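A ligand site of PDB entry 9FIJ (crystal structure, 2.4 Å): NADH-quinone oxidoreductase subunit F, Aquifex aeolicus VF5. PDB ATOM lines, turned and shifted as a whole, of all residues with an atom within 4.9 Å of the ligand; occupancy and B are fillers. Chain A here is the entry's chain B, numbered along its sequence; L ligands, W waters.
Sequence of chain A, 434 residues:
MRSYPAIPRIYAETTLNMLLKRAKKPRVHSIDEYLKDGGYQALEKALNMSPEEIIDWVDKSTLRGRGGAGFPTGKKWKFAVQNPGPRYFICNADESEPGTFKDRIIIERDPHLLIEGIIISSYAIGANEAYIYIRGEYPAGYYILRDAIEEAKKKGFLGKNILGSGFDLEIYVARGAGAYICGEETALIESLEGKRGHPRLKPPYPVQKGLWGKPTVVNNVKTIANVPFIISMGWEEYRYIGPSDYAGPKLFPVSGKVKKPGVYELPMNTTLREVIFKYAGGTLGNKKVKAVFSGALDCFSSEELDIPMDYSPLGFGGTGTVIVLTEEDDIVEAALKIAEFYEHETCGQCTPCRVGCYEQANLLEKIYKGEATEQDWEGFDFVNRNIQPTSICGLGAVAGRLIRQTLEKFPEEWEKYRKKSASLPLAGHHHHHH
The side-chain amide nitrogen (ND2) of Asn 220 lies within hydrogen-bond range of an oxygen (O1) of the ligand (2.9 Å). An oxygen (O8) of the ligand lies within hydrogen-bond range of the side-chain amide nitrogen (ND2) of Asn 219 (3.0 Å). The backbone NH of Glu 185 lies within hydrogen-bond range of an oxygen (O3) of the ligand. The backbone NH of Gly 67 is in hydrogen-bond range of an oxygen (O9) of the ligand, at 2.7 Å. N of Arg 66 sits at hydrogen-bond distance from O9 of the ligand. OG1 of Thr 223 lies within hydrogen-bond range of O8 of the ligand (2.7 Å). The backbone NH (N) of Glu 95 is in hydrogen-bond range of an oxygen (O2) of the ligand (3.1 Å). NZ of Lys 76 lies within salt-bridge range of O7 of the ligand (2.8 Å). The backbone NH of Asn 220 is in hydrogen-bond range of an oxygen (O8) of the ligand, at 2.7 Å. O5 of the ligand sits close to ND2 of Asn 92, 3.2 Å away.
The backbone NH (N) of Gly 65 lies within hydrogen-bond range of the backbone carbonyl oxygen (O) of Phe 71 (2.8 Å). OD1 of Asn 92 lies within hydrogen-bond range of N of Asp 94 (3.1 Å). O of Asn 219 sits at hydrogen-bond distance from N of Asn 92, 2.8 Å away. OD2 of Asp 94 sits at hydrogen-bond distance from N of Gly 183 (3.3 Å). The backbone carbonyl oxygen (O) of Val 218 is in hydrogen-bond range of the side-chain amino group (NZ) of Lys 76, at 2.8 Å. OG1 of Thr 223 lies within hydrogen-bond range of N of Arg 66 (2.8 Å). O of Asp 94 lies within hydrogen-bond range of OG of Ser 96 (2.8 Å). ND2 of Asn 92 is in hydrogen-bond range of O of Gly 183 (2.8 Å).
The backbone carbonyl oxygen (O) of Gly 183 sits close to a nitrogen (N1) of the ligand (3.3 Å). An oxygen (O6) of the ligand sits close to the backbone carbonyl oxygen of Val 218 (3.5 Å). Gly 65 touches the ligand. C of Asp 94 touches O2 of the ligand, 3.8 Å away. Tyr 180 touches the ligand. CD1 of Ile 181 touches C9 of the ligand (3.8 Å). Glu 184 touches the ligand (CA to O3, 3.5 Å). N of Gly 394 touches C11 of the ligand, at 3.9 Å. Hydrophobic or aromatic side chains within 4 Å of the ligand: Tyr 180 and Ile 181. Within 4 Å of the ligand: Gly 65, Arg 66, Gly 67, Lys 76, Asn 92, Asp 94, Glu 95, Tyr 180, Ile 181, Gly 183, Glu 184, Glu 185, Val 218, Asn 219, Asn 220, Thr 223 and Gly 394.
Water W2 lies within hydrogen-bond range of O9 of the ligand (2.4 Å), N of Ala 69 (2.9 Å) and N of Gly 68 (3.2 Å). Water W3 bridges O7 of the ligand (2.7 Å) and N of Phe 71 (3.0 Å). Water W6 lies within hydrogen-bond range of O of Phe 71 (2.8 Å), O7 of the ligand (2.8 Å), ND2 of Asn 219 (3.2 Å) and N of Gly 65 (3.4 Å).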
ATOM      1  N   GLY A  65      14.888  -0.187 -13.787  1.00  0.00           N
ATOM      2  CA  GLY A  65      15.256   0.646 -12.646  1.00  0.00           C
ATOM      3  C   GLY A  65      14.546   0.179 -11.372  1.00  0.00           C
ATOM      4  O   GLY A  65      13.349  -0.102 -11.395  1.00  0.00           O
ATOM      5  N   ARG A  66      15.279   0.123 -10.264  1.00  0.00           N
ATOM      6  CA  ARG A  66      14.785  -0.411  -9.011  1.00  0.00           C
ATOM      7  C   ARG A  66      14.362   0.723  -8.067  1.00  0.00           C
ATOM      8  O   ARG A  66      13.969   0.466  -6.943  1.00  0.00           O
ATOM      9  CB  ARG A  66      15.874  -1.228  -8.308  1.00  0.00           C
ATOM     10  CG  ARG A  66      16.330  -2.440  -9.106  1.00  0.00           C
ATOM     11  CD  ARG A  66      15.242  -3.470  -9.279  1.00  0.00           C
ATOM     12  NE  ARG A  66      15.794  -4.790  -9.616  1.00  0.00           N
ATOM     13  CZ  ARG A  66      15.590  -5.441 -10.752  1.00  0.00           C
ATOM     14  NH1 ARG A  66      15.919  -6.721 -10.854  1.00  0.00           N
ATOM     15  NH2 ARG A  66      15.003  -4.824 -11.767  1.00  0.00           N
ATOM     16  N   GLY A  67      14.428   1.977  -8.564  1.00  0.00           N
ATOM     17  CA  GLY A  67      14.099   3.145  -7.764  1.00  0.00           C
ATOM     18  C   GLY A  67      12.597   3.406  -7.670  1.00  0.00           C
ATOM     19  O   GLY A  67      12.200   4.274  -6.901  1.00  0.00           O
ATOM     20  N   GLY A  68      11.776   2.690  -8.445  1.00  0.00           N
ATOM     21  CA  GLY A  68      10.328   2.817  -8.351  1.00  0.00           C
ATOM     22  C   GLY A  68       9.663   2.867  -9.725  1.00  0.00           C
ATOM     23  O   GLY A  68       8.658   2.192  -9.938  1.00  0.00           O
ATOM     24  N   ALA A  69      10.232   3.639 -10.653  1.00  0.00           N
ATOM     25  CA  ALA A  69       9.597   3.942 -11.925  1.00  0.00           C
ATOM     26  C   ALA A  69       9.687   2.774 -12.895  1.00  0.00           C
ATOM     27  O   ALA A  69       8.900   2.715 -13.841  1.00  0.00           O
ATOM     28  CB  ALA A  69      10.207   5.190 -12.523  1.00  0.00           C
ATOM     29  N   PHE A  71      11.987   2.026 -15.154  1.00  0.00           N
ATOM     30  CA  PHE A  71      12.409   2.376 -16.505  1.00  0.00           C
ATOM     31  C   PHE A  71      13.589   1.485 -16.921  1.00  0.00           C
ATOM     32  O   PHE A  71      14.541   1.316 -16.164  1.00  0.00           O
ATOM     33  CB  PHE A  71      12.767   3.856 -16.635  1.00  0.00           C
ATOM     34  CG  PHE A  71      12.829   4.308 -18.089  1.00  0.00           C
ATOM     35  CD1 PHE A  71      11.691   4.796 -18.737  1.00  0.00           C
ATOM     36  CD2 PHE A  71      14.003   4.196 -18.830  1.00  0.00           C
ATOM     37  CE1 PHE A  71      11.741   5.161 -20.076  1.00  0.00           C
ATOM     38  CE2 PHE A  71      14.053   4.574 -20.162  1.00  0.00           C
ATOM     39  CZ  PHE A  71      12.919   5.054 -20.782  1.00  0.00           C
ATOM     40  N   LYS A  76      17.723   3.953 -21.087  1.00  0.00           N
ATOM     41  CA  LYS A  76      18.055   5.198 -20.412  1.00  0.00           C
ATOM     42  C   LYS A  76      19.492   5.603 -20.761  1.00  0.00           C
ATOM     43  O   LYS A  76      19.759   6.753 -21.108  1.00  0.00           O
ATOM     44  CB  LYS A  76      17.816   5.079 -18.907  1.00  0.00           C
ATOM     45  CG  LYS A  76      18.059   6.342 -18.110  1.00  0.00           C
ATOM     46  CD  LYS A  76      18.140   6.147 -16.598  1.00  0.00           C
ATOM     47  CE  LYS A  76      16.818   5.998 -15.937  1.00  0.00           C
ATOM     48  NZ  LYS A  76      16.953   6.223 -14.482  1.00  0.00           N
ATOM     49  N   ASN A  92      21.687   7.281  -6.797  1.00  0.00           N
ATOM     50  CA  ASN A  92      20.653   7.791  -5.916  1.00  0.00           C
ATOM     51  C   ASN A  92      20.616   6.922  -4.656  1.00  0.00           C
ATOM     52  O   ASN A  92      20.111   5.794  -4.685  1.00  0.00           O
ATOM     53  CB  ASN A  92      19.312   7.841  -6.622  1.00  0.00           C
ATOM     54  CG  ASN A  92      18.274   8.601  -5.833  1.00  0.00           C
ATOM     55  OD1 ASN A  92      18.441   8.808  -4.624  1.00  0.00           O
ATOM     56  ND2 ASN A  92      17.195   9.020  -6.483  1.00  0.00           N
ATOM     57  N   ASP A  94      19.182   8.145  -1.649  1.00  0.00           N
ATOM     58  CA  ASP A  94      18.437   9.027  -0.760  1.00  0.00           C
ATOM     59  C   ASP A  94      17.503   8.262   0.181  1.00  0.00           C
ATOM     60  O   ASP A  94      17.249   8.737   1.287  1.00  0.00           O
ATOM     61  CB  ASP A  94      17.676  10.106  -1.501  1.00  0.00           C
ATOM     62  CG  ASP A  94      17.293  11.245  -0.561  1.00  0.00           C
ATOM     63  OD1 ASP A  94      18.230  11.890  -0.061  1.00  0.00           O
ATOM     64  OD2 ASP A  94      16.077  11.405  -0.285  1.00  0.00           O
ATOM     65  N   GLU A  95      16.973   7.122  -0.289  1.00  0.00           N
ATOM     66  CA  GLU A  95      16.144   6.198   0.479  1.00  0.00           C
ATOM     67  C   GLU A  95      15.554   6.848   1.737  1.00  0.00           C
ATOM     68  O   GLU A  95      16.076   6.637   2.844  1.00  0.00           O
ATOM     69  CB  GLU A  95      16.955   4.954   0.830  1.00  0.00           C
ATOM     70  CG  GLU A  95      16.107   3.829   1.403  1.00  0.00           C
ATOM     71  CD  GLU A  95      16.800   2.502   1.614  1.00  0.00           C
ATOM     72  OE1 GLU A  95      17.765   2.396   2.433  1.00  0.00           O
ATOM     73  OE2 GLU A  95      16.336   1.569   0.930  1.00  0.00           O
ATOM     74  N   SER A  96      14.471   7.606   1.546  1.00  0.00           N
ATOM     75  CA  SER A  96      13.769   8.274   2.641  1.00  0.00           C
ATOM     76  C   SER A  96      12.280   7.896   2.696  1.00  0.00           C
ATOM     77  O   SER A  96      11.566   8.403   3.554  1.00  0.00           O
ATOM     78  CB  SER A  96      13.951   9.777   2.556  1.00  0.00           C
ATOM     79  OG  SER A  96      15.320  10.153   2.672  1.00  0.00           O
ATOM     80  N   TYR A 180      12.857  14.299   1.834  1.00  0.00           N
ATOM     81  CA  TYR A 180      12.442  13.136   1.074  1.00  0.00           C
ATOM     82  C   TYR A 180      12.462  13.468  -0.415  1.00  0.00           C
ATOM     83  O   TYR A 180      12.711  12.576  -1.227  1.00  0.00           O
ATOM     84  CB  TYR A 180      11.035  12.709   1.510  1.00  0.00           C
ATOM     85  CG  TYR A 180      10.349  11.698   0.609  1.00  0.00           C
ATOM     86  CD1 TYR A 180      10.875  10.430   0.398  1.00  0.00           C
ATOM     87  CD2 TYR A 180       9.119  11.985   0.010  1.00  0.00           C
ATOM     88  CE1 TYR A 180      10.246   9.504  -0.417  1.00  0.00           C
ATOM     89  CE2 TYR A 180       8.466  11.067  -0.792  1.00  0.00           C
ATOM     90  CZ  TYR A 180       9.043   9.825  -1.001  1.00  0.00           C
ATOM     91  OH  TYR A 180       8.406   8.920  -1.781  1.00  0.00           O
ATOM     92  N   ILE A 181      12.160  14.737  -0.750  1.00  0.00           N
ATOM     93  CA  ILE A 181      11.940  15.137  -2.134  1.00  0.00           C
ATOM     94  C   ILE A 181      13.249  15.059  -2.910  1.00  0.00           C
ATOM     95  O   ILE A 181      13.203  14.927  -4.128  1.00  0.00           O
ATOM     96  CB  ILE A 181      11.299  16.533  -2.258  1.00  0.00           C
ATOM     97  CG1 ILE A 181      10.755  16.780  -3.673  1.00  0.00           C
ATOM     98  CG2 ILE A 181      12.256  17.645  -1.847  1.00  0.00           C
ATOM     99  CD1 ILE A 181       9.718  15.767  -4.141  1.00  0.00           C
ATOM    100  N   GLY A 183      15.091  12.686  -3.219  1.00  0.00           N
ATOM    101  CA  GLY A 183      15.171  11.407  -3.897  1.00  0.00           C
ATOM    102  C   GLY A 183      14.636  11.487  -5.327  1.00  0.00           C
ATOM    103  O   GLY A 183      14.966  10.640  -6.157  1.00  0.00           O
ATOM    104  N   GLU A 184      13.762  12.478  -5.604  1.00  0.00           N
ATOM    105  CA  GLU A 184      13.295  12.724  -6.964  1.00  0.00           C
ATOM    106  C   GLU A 184      14.487  13.215  -7.790  1.00  0.00           C
ATOM    107  O   GLU A 184      15.214  14.088  -7.330  1.00  0.00           O
ATOM    108  CB  GLU A 184      12.088  13.665  -6.969  1.00  0.00           C
ATOM    109  CG  GLU A 184      11.309  13.723  -8.279  1.00  0.00           C
ATOM    110  CD  GLU A 184      11.863  14.621  -9.381  1.00  0.00           C
ATOM    111  OE1 GLU A 184      12.725  15.461  -9.054  1.00  0.00           O
ATOM    112  OE2 GLU A 184      11.449  14.485 -10.551  1.00  0.00           O
ATOM    113  N   GLU A 185      14.713  12.627  -8.973  1.00  0.00           N
ATOM    114  CA  GLU A 185      15.975  12.753  -9.701  1.00  0.00           C
ATOM    115  C   GLU A 185      16.342  14.218  -9.979  1.00  0.00           C
ATOM    116  O   GLU A 185      17.505  14.584  -9.791  1.00  0.00           O
ATOM    117  CB  GLU A 185      16.013  11.875 -10.944  1.00  0.00           C
ATOM    118  CG  GLU A 185      14.841  12.043 -11.898  1.00  0.00           C
ATOM    119  CD  GLU A 185      15.024  11.304 -13.207  1.00  0.00           C
ATOM    120  OE1 GLU A 185      14.132  11.385 -14.078  1.00  0.00           O
ATOM    121  OE2 GLU A 185      16.073  10.647 -13.339  1.00  0.00           O
ATOM    122  N   VAL A 218      20.781   9.200 -13.684  1.00  0.00           N
ATOM    123  CA  VAL A 218      20.517   8.920 -12.282  1.00  0.00           C
ATOM    124  C   VAL A 218      19.977   7.488 -12.213  1.00  0.00           C
ATOM    125  O   VAL A 218      19.023   7.127 -12.899  1.00  0.00           O
ATOM    126  CB  VAL A 218      19.525   9.914 -11.652  1.00  0.00           C
ATOM    127  CG1 VAL A 218      19.381   9.715 -10.153  1.00  0.00           C
ATOM    128  CG2 VAL A 218      19.886  11.387 -11.917  1.00  0.00           C
ATOM    129  N   ASN A 219      20.643   6.654 -11.400  1.00  0.00           N
ATOM    130  CA  ASN A 219      20.219   5.281 -11.178  1.00  0.00           C
ATOM    131  C   ASN A 219      20.244   4.995  -9.680  1.00  0.00           C
ATOM    132  O   ASN A 219      21.088   5.527  -8.949  1.00  0.00           O
ATOM    133  CB  ASN A 219      21.086   4.274 -11.928  1.00  0.00           C
ATOM    134  CG  ASN A 219      20.625   4.024 -13.338  1.00  0.00           C
ATOM    135  OD1 ASN A 219      21.410   4.096 -14.292  1.00  0.00           O
ATOM    136  ND2 ASN A 219      19.357   3.681 -13.505  1.00  0.00           N
ATOM    137  N   ASN A 220      19.314   4.134  -9.261  1.00  0.00           N
ATOM    138  CA  ASN A 220      19.199   3.712  -7.882  1.00  0.00           C
ATOM    139  C   ASN A 220      20.357   2.772  -7.539  1.00  0.00           C
ATOM    140  O   ASN A 220      20.780   1.991  -8.393  1.00  0.00           O
ATOM    141  CB  ASN A 220      17.836   3.068  -7.649  1.00  0.00           C
ATOM    142  CG  ASN A 220      17.713   2.442  -6.280  1.00  0.00           C
ATOM    143  OD1 ASN A 220      17.705   1.215  -6.171  1.00  0.00           O
ATOM    144  ND2 ASN A 220      17.636   3.265  -5.236  1.00  0.00           N
ATOM    145  N   THR A 223      19.840  -0.740  -8.712  1.00  0.00           N
ATOM    146  CA  THR A 223      19.946  -0.863 -10.155  1.00  0.00           C
ATOM    147  C   THR A 223      21.422  -1.025 -10.508  1.00  0.00           C
ATOM    148  O   THR A 223      21.785  -1.882 -11.300  1.00  0.00           O
ATOM    149  CB  THR A 223      19.360   0.346 -10.867  1.00  0.00           C
ATOM    150  OG1 THR A 223      18.062   0.565 -10.306  1.00  0.00           O
ATOM    151  CG2 THR A 223      19.257   0.140 -12.370  1.00  0.00           C
ATOM    152  N   CYS A 393       5.677  16.862 -10.089  1.00  0.00           N
ATOM    153  CA  CYS A 393       6.415  15.666  -9.716  1.00  0.00           C
ATOM    154  C   CYS A 393       5.496  14.657  -9.037  1.00  0.00           C
ATOM    155  O   CYS A 393       4.340  14.937  -8.752  1.00  0.00           O
ATOM    156  CB  CYS A 393       7.624  16.003  -8.844  1.00  0.00           C
ATOM    157  SG  CYS A 393       7.318  15.879  -7.066  1.00  0.00           S
ATOM    158  N   GLY A 394       6.039  13.460  -8.781  1.00  0.00           N
ATOM    159  CA  GLY A 394       5.228  12.309  -8.425  1.00  0.00           C
ATOM    160  C   GLY A 394       4.582  12.418  -7.035  1.00  0.00           C
ATOM    161  O   GLY A 394       3.543  11.811  -6.812  1.00  0.00           O
ATOM    162  N   LEU A 395       5.196  13.179  -6.125  1.00  0.00           N
ATOM    163  CA  LEU A 395       4.725  13.254  -4.745  1.00  0.00           C
ATOM    164  C   LEU A 395       3.289  13.773  -4.675  1.00  0.00           C
ATOM    165  O   LEU A 395       2.452  13.211  -3.967  1.00  0.00           O
ATOM    166  CB  LEU A 395       5.679  14.120  -3.924  1.00  0.00           C
ATOM    167  CG  LEU A 395       5.403  14.197  -2.426  1.00  0.00           C
ATOM    168  CD1 LEU A 395       6.663  14.541  -1.636  1.00  0.00           C
ATOM    169  CD2 LEU A 395       4.296  15.198  -2.101  1.00  0.00           C
HETATM  170  C1  LIG L   1      11.776   9.128  -6.154  1.00  0.00           C
HETATM  171  N1  LIG L   1      12.741   8.229  -6.738  1.00  0.00           N
HETATM  172  C2  LIG L   1      13.689   7.666  -5.894  1.00  0.00           C
HETATM  173  N2  LIG L   1      14.667   6.878  -6.445  1.00  0.00           N
HETATM  174  C3  LIG L   1      15.720   6.383  -5.717  1.00  0.00           C
HETATM  175  O1  LIG L   1      16.664   5.783  -6.246  1.00  0.00           O
HETATM  176  N3  LIG L   1      15.680   6.648  -4.365  1.00  0.00           N
HETATM  177  C4  LIG L   1      14.724   7.411  -3.692  1.00  0.00           C
HETATM  178  O2  LIG L   1      14.804   7.592  -2.473  1.00  0.00           O
HETATM  179  C5  LIG L   1      13.719   7.932  -4.538  1.00  0.00           C
HETATM  180  N4  LIG L   1      12.822   8.790  -4.005  1.00  0.00           N
HETATM  181  C6  LIG L   1      11.874   9.420  -4.781  1.00  0.00           C
HETATM  182  C7  LIG L   1      11.013  10.333  -4.197  1.00  0.00           C
HETATM  183  C8  LIG L   1      10.029  10.975  -4.954  1.00  0.00           C
HETATM  184  C9  LIG L   1       9.121  11.972  -4.276  1.00  0.00           C
HETATM  185  C10 LIG L   1       9.920  10.687  -6.320  1.00  0.00           C
HETATM  186  C11 LIG L   1       8.836  11.326  -7.154  1.00  0.00           C
HETATM  187  C12 LIG L   1      10.792   9.770  -6.910  1.00  0.00           C
HETATM  188  C13 LIG L   1      12.751   7.961  -8.176  1.00  0.00           C
HETATM  189  C14 LIG L   1      13.849   8.752  -8.882  1.00  0.00           C
HETATM  190  O3  LIG L   1      13.340  10.041  -9.244  1.00  0.00           O
HETATM  191  C15 LIG L   1      14.308   8.030 -10.153  1.00  0.00           C
HETATM  192  O4  LIG L   1      13.202   7.483 -10.850  1.00  0.00           O
HETATM  193  C16 LIG L   1      15.291   6.880  -9.901  1.00  0.00           C
HETATM  194  O5  LIG L   1      16.285   7.228  -8.936  1.00  0.00           O
HETATM  195  C17 LIG L   1      15.987   6.469 -11.173  1.00  0.00           C
HETATM  196  O6  LIG L   1      16.810   5.342 -10.875  1.00  0.00           O
HETATM  197  P1  LIG L   1      16.409   3.890 -11.484  1.00  0.00           P
HETATM  198  O7  LIG L   1      16.159   4.050 -12.963  1.00  0.00           O
HETATM  199  O8  LIG L   1      17.653   3.085 -11.162  1.00  0.00           O
HETATM  200  O9  LIG L   1      15.176   3.388 -10.745  1.00  0.00           O
HETATM  201  O   HOH W   1      12.984   5.124  -1.009  1.00  0.00           O
HETATM  202  O   HOH W   2      13.027   4.486 -10.726  1.00  0.00           O
HETATM  203  O   HOH W   3      13.525   3.913 -13.459  1.00  0.00           O
HETATM  204  O   HOH W   4      17.951   5.578  -2.953  1.00  0.00           O
HETATM  205  O   HOH W   5      13.744   9.776  -1.134  1.00  0.00           O
HETATM  206  O   HOH W   6      16.909   2.294 -15.034  1.00  0.00           O
